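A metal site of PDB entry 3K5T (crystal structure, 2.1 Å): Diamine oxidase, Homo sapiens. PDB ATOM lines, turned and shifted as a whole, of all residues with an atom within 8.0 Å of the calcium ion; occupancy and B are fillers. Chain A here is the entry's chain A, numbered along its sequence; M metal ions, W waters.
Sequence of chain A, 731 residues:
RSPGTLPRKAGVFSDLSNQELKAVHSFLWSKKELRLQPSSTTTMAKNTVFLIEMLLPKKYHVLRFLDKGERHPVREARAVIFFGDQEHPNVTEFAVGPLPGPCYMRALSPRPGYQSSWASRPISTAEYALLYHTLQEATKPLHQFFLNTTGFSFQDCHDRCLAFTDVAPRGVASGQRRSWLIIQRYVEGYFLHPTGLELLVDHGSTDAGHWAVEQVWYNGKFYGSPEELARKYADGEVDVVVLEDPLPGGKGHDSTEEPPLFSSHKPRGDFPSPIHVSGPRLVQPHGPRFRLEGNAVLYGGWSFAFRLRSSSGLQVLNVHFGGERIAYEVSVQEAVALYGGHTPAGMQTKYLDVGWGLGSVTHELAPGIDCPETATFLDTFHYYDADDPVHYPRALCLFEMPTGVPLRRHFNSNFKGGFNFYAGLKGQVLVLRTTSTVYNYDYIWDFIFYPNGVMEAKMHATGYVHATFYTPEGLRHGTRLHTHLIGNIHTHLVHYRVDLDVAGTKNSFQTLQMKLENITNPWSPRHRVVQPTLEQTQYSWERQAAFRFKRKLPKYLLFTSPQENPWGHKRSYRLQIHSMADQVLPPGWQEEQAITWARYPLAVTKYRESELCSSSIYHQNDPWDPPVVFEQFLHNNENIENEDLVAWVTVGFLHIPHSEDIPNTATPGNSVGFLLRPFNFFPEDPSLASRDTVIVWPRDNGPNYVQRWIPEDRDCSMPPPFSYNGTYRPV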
ATOM      1  N   GLU A 542      12.448  17.598 -30.186  1.00  0.00           N
ATOM      2  CA  GLU A 542      13.643  18.348 -29.707  1.00  0.00           C
ATOM      3  C   GLU A 542      14.577  17.495 -28.865  1.00  0.00           C
ATOM      4  O   GLU A 542      15.763  17.373 -29.176  1.00  0.00           O
ATOM      5  CB  GLU A 542      13.229  19.543 -28.883  1.00  0.00           C
ATOM      6  CG  GLU A 542      12.927  20.756 -29.693  1.00  0.00           C
ATOM      7  CD  GLU A 542      12.235  21.820 -28.885  1.00  0.00           C
ATOM      8  OE1 GLU A 542      11.690  21.523 -27.809  1.00  0.00           O
ATOM      9  OE2 GLU A 542      12.222  22.966 -29.328  1.00  0.00           O
ATOM     10  N   ARG A 543      14.022  16.912 -27.803  1.00  0.00           N
ATOM     11  CA  ARG A 543      14.764  16.059 -26.873  1.00  0.00           C
ATOM     12  C   ARG A 543      15.556  14.921 -27.530  1.00  0.00           C
ATOM     13  O   ARG A 543      16.584  14.491 -27.005  1.00  0.00           O
ATOM     14  CB  ARG A 543      13.805  15.496 -25.820  1.00  0.00           C
ATOM     15  CG  ARG A 543      14.428  14.548 -24.820  1.00  0.00           C
ATOM     16  CD  ARG A 543      15.644  15.147 -24.116  1.00  0.00           C
ATOM     17  NE  ARG A 543      15.304  16.358 -23.370  1.00  0.00           N
ATOM     18  CZ  ARG A 543      16.197  17.111 -22.715  1.00  0.00           C
ATOM     19  NH1 ARG A 543      17.490  16.794 -22.713  1.00  0.00           N
ATOM     20  NH2 ARG A 543      15.766  18.193 -22.056  1.00  0.00           N
ATOM     21  N   VAL A 604      19.401  20.845 -30.835  1.00  0.00           N
ATOM     22  CA  VAL A 604      18.561  21.398 -31.901  1.00  0.00           C
ATOM     23  C   VAL A 604      17.248  21.902 -31.298  1.00  0.00           C
ATOM     24  O   VAL A 604      16.498  21.131 -30.668  1.00  0.00           O
ATOM     25  CB  VAL A 604      18.230  20.350 -32.986  1.00  0.00           C
ATOM     26  CG1 VAL A 604      17.417  20.987 -34.124  1.00  0.00           C
ATOM     27  CG2 VAL A 604      19.512  19.694 -33.533  1.00  0.00           C
ATOM     28  N   THR A 605      16.965  23.187 -31.448  1.00  0.00           N
ATOM     29  CA  THR A 605      15.660  23.693 -31.062  1.00  0.00           C
ATOM     30  C   THR A 605      14.848  24.183 -32.251  1.00  0.00           C
ATOM     31  O   THR A 605      15.363  24.410 -33.361  1.00  0.00           O
ATOM     32  CB  THR A 605      15.723  24.786 -29.986  1.00  0.00           C
ATOM     33  OG1 THR A 605      16.348  25.952 -30.514  1.00  0.00           O
ATOM     34  CG2 THR A 605      16.477  24.277 -28.746  1.00  0.00           C
ATOM     35  N   LYS A 606      13.553  24.297 -32.021  1.00  0.00           N
ATOM     36  CA  LYS A 606      12.646  24.894 -32.968  1.00  0.00           C
ATOM     37  C   LYS A 606      12.726  26.388 -32.680  1.00  0.00           C
ATOM     38  O   LYS A 606      12.718  26.813 -31.523  1.00  0.00           O
ATOM     39  CB  LYS A 606      11.245  24.343 -32.734  1.00  0.00           C
ATOM     40  CG  LYS A 606      10.136  24.945 -33.560  1.00  0.00           C
ATOM     41  CD  LYS A 606       8.971  23.973 -33.630  1.00  0.00           C
ATOM     42  CE  LYS A 606       7.620  24.665 -33.604  1.00  0.00           C
ATOM     43  NZ  LYS A 606       6.584  23.686 -33.157  1.00  0.00           N
ATOM     44  N   TYR A 607      12.844  27.176 -33.755  1.00  0.00           N
ATOM     45  CA  TYR A 607      13.117  28.591 -33.665  1.00  0.00           C
ATOM     46  C   TYR A 607      12.022  29.330 -32.885  1.00  0.00           C
ATOM     47  O   TYR A 607      10.844  29.003 -33.028  1.00  0.00           O
ATOM     48  CB  TYR A 607      13.229  29.210 -35.080  1.00  0.00           C
ATOM     49  CG  TYR A 607      13.427  30.703 -35.032  1.00  0.00           C
ATOM     50  CD1 TYR A 607      12.331  31.579 -34.896  1.00  0.00           C
ATOM     51  CD2 TYR A 607      14.699  31.242 -35.052  1.00  0.00           C
ATOM     52  CE1 TYR A 607      12.516  32.945 -34.813  1.00  0.00           C
ATOM     53  CE2 TYR A 607      14.895  32.609 -34.979  1.00  0.00           C
ATOM     54  CZ  TYR A 607      13.820  33.449 -34.849  1.00  0.00           C
ATOM     55  OH  TYR A 607      14.072  34.790 -34.760  1.00  0.00           O
ATOM     56  N   ARG A 608      12.403  30.322 -32.087  1.00  0.00           N
ATOM     57  CA  ARG A 608      11.421  31.183 -31.421  1.00  0.00           C
ATOM     58  C   ARG A 608      12.050  32.500 -30.982  1.00  0.00           C
ATOM     59  O   ARG A 608      13.218  32.534 -30.548  1.00  0.00           O
ATOM     60  CB  ARG A 608      10.823  30.465 -30.204  1.00  0.00           C
ATOM     61  N   GLU A 611      13.810  32.706 -27.589  1.00  0.00           N
ATOM     62  CA  GLU A 611      14.983  31.848 -27.345  1.00  0.00           C
ATOM     63  C   GLU A 611      16.128  32.203 -28.314  1.00  0.00           C
ATOM     64  O   GLU A 611      16.816  31.335 -28.862  1.00  0.00           O
ATOM     65  CB  GLU A 611      14.594  30.384 -27.498  1.00  0.00           C
ATOM     66  CG  GLU A 611      13.308  30.007 -26.738  1.00  0.00           C
ATOM     67  CD  GLU A 611      12.950  28.524 -26.819  1.00  0.00           C
ATOM     68  OE1 GLU A 611      13.406  27.828 -27.756  1.00  0.00           O
ATOM     69  OE2 GLU A 611      12.195  28.054 -25.945  1.00  0.00           O
ATOM     70  N   PHE A 630      19.088  27.518 -20.770  1.00  0.00           N
ATOM     71  CA  PHE A 630      18.983  26.830 -22.049  1.00  0.00           C
ATOM     72  C   PHE A 630      18.218  25.507 -21.943  1.00  0.00           C
ATOM     73  O   PHE A 630      17.534  25.111 -22.882  1.00  0.00           O
ATOM     74  CB  PHE A 630      20.373  26.587 -22.633  1.00  0.00           C
ATOM     75  CG  PHE A 630      20.358  25.820 -23.934  1.00  0.00           C
ATOM     76  CD1 PHE A 630      20.057  26.466 -25.131  1.00  0.00           C
ATOM     77  CD2 PHE A 630      20.629  24.462 -23.965  1.00  0.00           C
ATOM     78  CE1 PHE A 630      20.034  25.784 -26.320  1.00  0.00           C
ATOM     79  CE2 PHE A 630      20.596  23.762 -25.166  1.00  0.00           C
ATOM     80  CZ  PHE A 630      20.299  24.433 -26.348  1.00  0.00           C
ATOM     81  N   GLU A 631      18.354  24.828 -20.814  1.00  0.00           N
ATOM     82  CA  GLU A 631      17.626  23.569 -20.585  1.00  0.00           C
ATOM     83  C   GLU A 631      16.128  23.762 -20.794  1.00  0.00           C
ATOM     84  O   GLU A 631      15.473  22.879 -21.338  1.00  0.00           O
ATOM     85  CB  GLU A 631      17.893  23.040 -19.171  1.00  0.00           C
ATOM     86  CG  GLU A 631      17.258  21.664 -18.864  1.00  0.00           C
ATOM     87  CD  GLU A 631      17.836  20.547 -19.724  1.00  0.00           C
ATOM     88  OE1 GLU A 631      18.995  20.696 -20.158  1.00  0.00           O
ATOM     89  OE2 GLU A 631      17.130  19.537 -19.953  1.00  0.00           O
ATOM     90  N   GLN A 632      15.586  24.906 -20.379  1.00  0.00           N
ATOM     91  CA  GLN A 632      14.151  25.218 -20.503  1.00  0.00           C
ATOM     92  C   GLN A 632      13.653  25.240 -21.951  1.00  0.00           C
ATOM     93  O   GLN A 632      12.501  24.854 -22.229  1.00  0.00           O
ATOM     94  CB  GLN A 632      13.833  26.545 -19.847  1.00  0.00           C
ATOM     95  N   PHE A 633      14.514  25.671 -22.872  1.00  0.00           N
ATOM     96  CA  PHE A 633      14.223  25.619 -24.307  1.00  0.00           C
ATOM     97  C   PHE A 633      13.731  24.227 -24.741  1.00  0.00           C
ATOM     98  O   PHE A 633      12.895  24.115 -25.642  1.00  0.00           O
ATOM     99  CB  PHE A 633      15.470  25.978 -25.136  1.00  0.00           C
ATOM    100  CG  PHE A 633      15.955  27.408 -24.997  1.00  0.00           C
ATOM    101  CD1 PHE A 633      15.238  28.377 -24.285  1.00  0.00           C
ATOM    102  CD2 PHE A 633      17.124  27.800 -25.642  1.00  0.00           C
ATOM    103  CE1 PHE A 633      15.709  29.687 -24.192  1.00  0.00           C
ATOM    104  CE2 PHE A 633      17.591  29.103 -25.543  1.00  0.00           C
ATOM    105  CZ  PHE A 633      16.882  30.051 -24.831  1.00  0.00           C
ATOM    106  N   LEU A 634      14.269  23.181 -24.117  1.00  0.00           N
ATOM    107  CA  LEU A 634      13.918  21.817 -24.488  1.00  0.00           C
ATOM    108  C   LEU A 634      12.677  21.285 -23.770  1.00  0.00           C
ATOM    109  O   LEU A 634      12.156  20.240 -24.151  1.00  0.00           O
ATOM    110  CB  LEU A 634      15.101  20.886 -24.217  1.00  0.00           C
ATOM    111  CG  LEU A 634      16.405  21.159 -24.961  1.00  0.00           C
ATOM    112  CD1 LEU A 634      17.494  20.197 -24.488  1.00  0.00           C
ATOM    113  CD2 LEU A 634      16.233  21.036 -26.471  1.00  0.00           C
ATOM    114  N   HIS A 635      12.187  22.011 -22.775  1.00  0.00           N
ATOM    115  CA  HIS A 635      11.112  21.536 -21.905  1.00  0.00           C
ATOM    116  C   HIS A 635       9.802  21.198 -22.622  1.00  0.00           C
ATOM    117  O   HIS A 635       9.190  20.176 -22.333  1.00  0.00           O
ATOM    118  CB  HIS A 635      10.818  22.552 -20.810  1.00  0.00           C
ATOM    119  CG  HIS A 635       9.873  22.062 -19.764  1.00  0.00           C
ATOM    120  ND1 HIS A 635       8.647  22.650 -19.532  1.00  0.00           N
ATOM    121  CD2 HIS A 635       9.973  21.023 -18.896  1.00  0.00           C
ATOM    122  CE1 HIS A 635       8.036  21.998 -18.561  1.00  0.00           C
ATOM    123  NE2 HIS A 635       8.820  21.014 -18.153  1.00  0.00           N
ATOM    124  N   ASN A 636       9.375  22.048 -23.542  1.00  0.00           N
ATOM    125  CA  ASN A 636       8.154  21.731 -24.284  1.00  0.00           C
ATOM    126  C   ASN A 636       8.381  20.655 -25.348  1.00  0.00           C
ATOM    127  O   ASN A 636       7.440  20.268 -26.031  1.00  0.00           O
ATOM    128  CB  ASN A 636       7.490  22.986 -24.869  1.00  0.00           C
ATOM    129  CG  ASN A 636       8.439  23.829 -25.706  1.00  0.00           C
ATOM    130  OD1 ASN A 636       9.605  23.477 -25.919  1.00  0.00           O
ATOM    131  ND2 ASN A 636       7.936  24.967 -26.175  1.00  0.00           N
ATOM    132  N   ASN A 637       9.623  20.157 -25.462  1.00  0.00           N
ATOM    133  CA  ASN A 637       9.998  19.088 -26.396  1.00  0.00           C
ATOM    134  C   ASN A 637       9.108  19.102 -27.632  1.00  0.00           C
ATOM    135  O   ASN A 637       8.236  18.247 -27.813  1.00  0.00           O
ATOM    136  CB  ASN A 637       9.965  17.722 -25.707  1.00  0.00           C
ATOM    137  CG  ASN A 637      10.607  16.616 -26.555  1.00  0.00           C
ATOM    138  OD1 ASN A 637      11.393  16.888 -27.463  1.00  0.00           O
ATOM    139  ND2 ASN A 637      10.283  15.380 -26.249  1.00  0.00           N
ATOM    140  N   GLU A 638       9.321  20.123 -28.457  1.00  0.00           N
ATOM    141  CA  GLU A 638       8.519  20.357 -29.658  1.00  0.00           C
ATOM    142  C   GLU A 638       8.990  19.489 -30.820  1.00  0.00           C
ATOM    143  O   GLU A 638      10.142  19.051 -30.866  1.00  0.00           O
ATOM    144  CB  GLU A 638       8.585  21.822 -30.047  1.00  0.00           C
ATOM    145  CG  GLU A 638       7.857  22.728 -29.085  1.00  0.00           C
ATOM    146  CD  GLU A 638       8.162  24.191 -29.298  1.00  0.00           C
ATOM    147  OE1 GLU A 638       9.351  24.569 -29.349  1.00  0.00           O
ATOM    148  OE2 GLU A 638       7.190  24.966 -29.389  1.00  0.00           O
ATOM    149  N   ASN A 639       8.071  19.264 -31.766  1.00  0.00           N
ATOM    150  CA  ASN A 639       8.338  18.480 -32.960  1.00  0.00           C
ATOM    151  C   ASN A 639       9.258  19.256 -33.899  1.00  0.00           C
ATOM    152  O   ASN A 639       9.050  20.447 -34.134  1.00  0.00           O
ATOM    153  CB  ASN A 639       7.020  18.115 -33.663  1.00  0.00           C
ATOM    154  CG  ASN A 639       7.200  17.739 -35.130  1.00  0.00           C
ATOM    155  OD1 ASN A 639       6.954  18.554 -36.014  1.00  0.00           O
ATOM    156  ND2 ASN A 639       7.656  16.511 -35.400  1.00  0.00           N
ATOM    157  N   ILE A 640      10.276  18.578 -34.424  1.00  0.00           N
ATOM    158  CA  ILE A 640      11.283  19.199 -35.282  1.00  0.00           C
ATOM    159  C   ILE A 640      11.313  18.625 -36.703  1.00  0.00           C
ATOM    160  O   ILE A 640      12.364  18.606 -37.369  1.00  0.00           O
ATOM    161  CB  ILE A 640      12.692  19.131 -34.630  1.00  0.00           C
ATOM    162  CG1 ILE A 640      13.117  17.674 -34.374  1.00  0.00           C
ATOM    163  CG2 ILE A 640      12.707  19.937 -33.354  1.00  0.00           C
ATOM    164  CD1 ILE A 640      14.459  17.554 -33.680  1.00  0.00           C
HETATM  165 CA    CA M   1      11.245  23.992 -27.398  1.00  0.00          CA
HETATM  166  O   HOH W   1      10.532  25.861 -26.007  1.00  0.00           O
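The backbone NH (N) of Lys 606 lies close to the side-chain carboxylate (OE2) of Glu 542 (3.3 Å). The side-chain amide oxygen (OD1) of Asn 637 lies within hydrogen-bond range of the backbone NH (N) of Glu 542 (3.0 Å).
Four residues have an atom within 4 Å of the calcium ion: Glu 542, Phe 633, Asn 636 and Glu 638. The nearest printed residue that does not touch the calcium ion is Glu 611 (4.4 Å).
The calcium ion is bound by the side-chain amide oxygen (OD1) of Asn 636 (2.3 Å), the side-chain carboxylate (OE2) of Glu 542 (2.4 Å), the backbone carbonyl oxygen (O) of Phe 633 (2.4 Å), water W1 (2.4 Å), the side-chain carboxylate (OE1) of Glu 542 (2.5 Å) and the side-chain carboxylate (OE1) of Glu 638 (2.8 Å).
Water W1 bridges the side-chain amide nitrogen (ND2) of Asn 636 (2.8 Å) and the side-chain carboxylate (OE2) of Glu 611 (2.8 Å).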
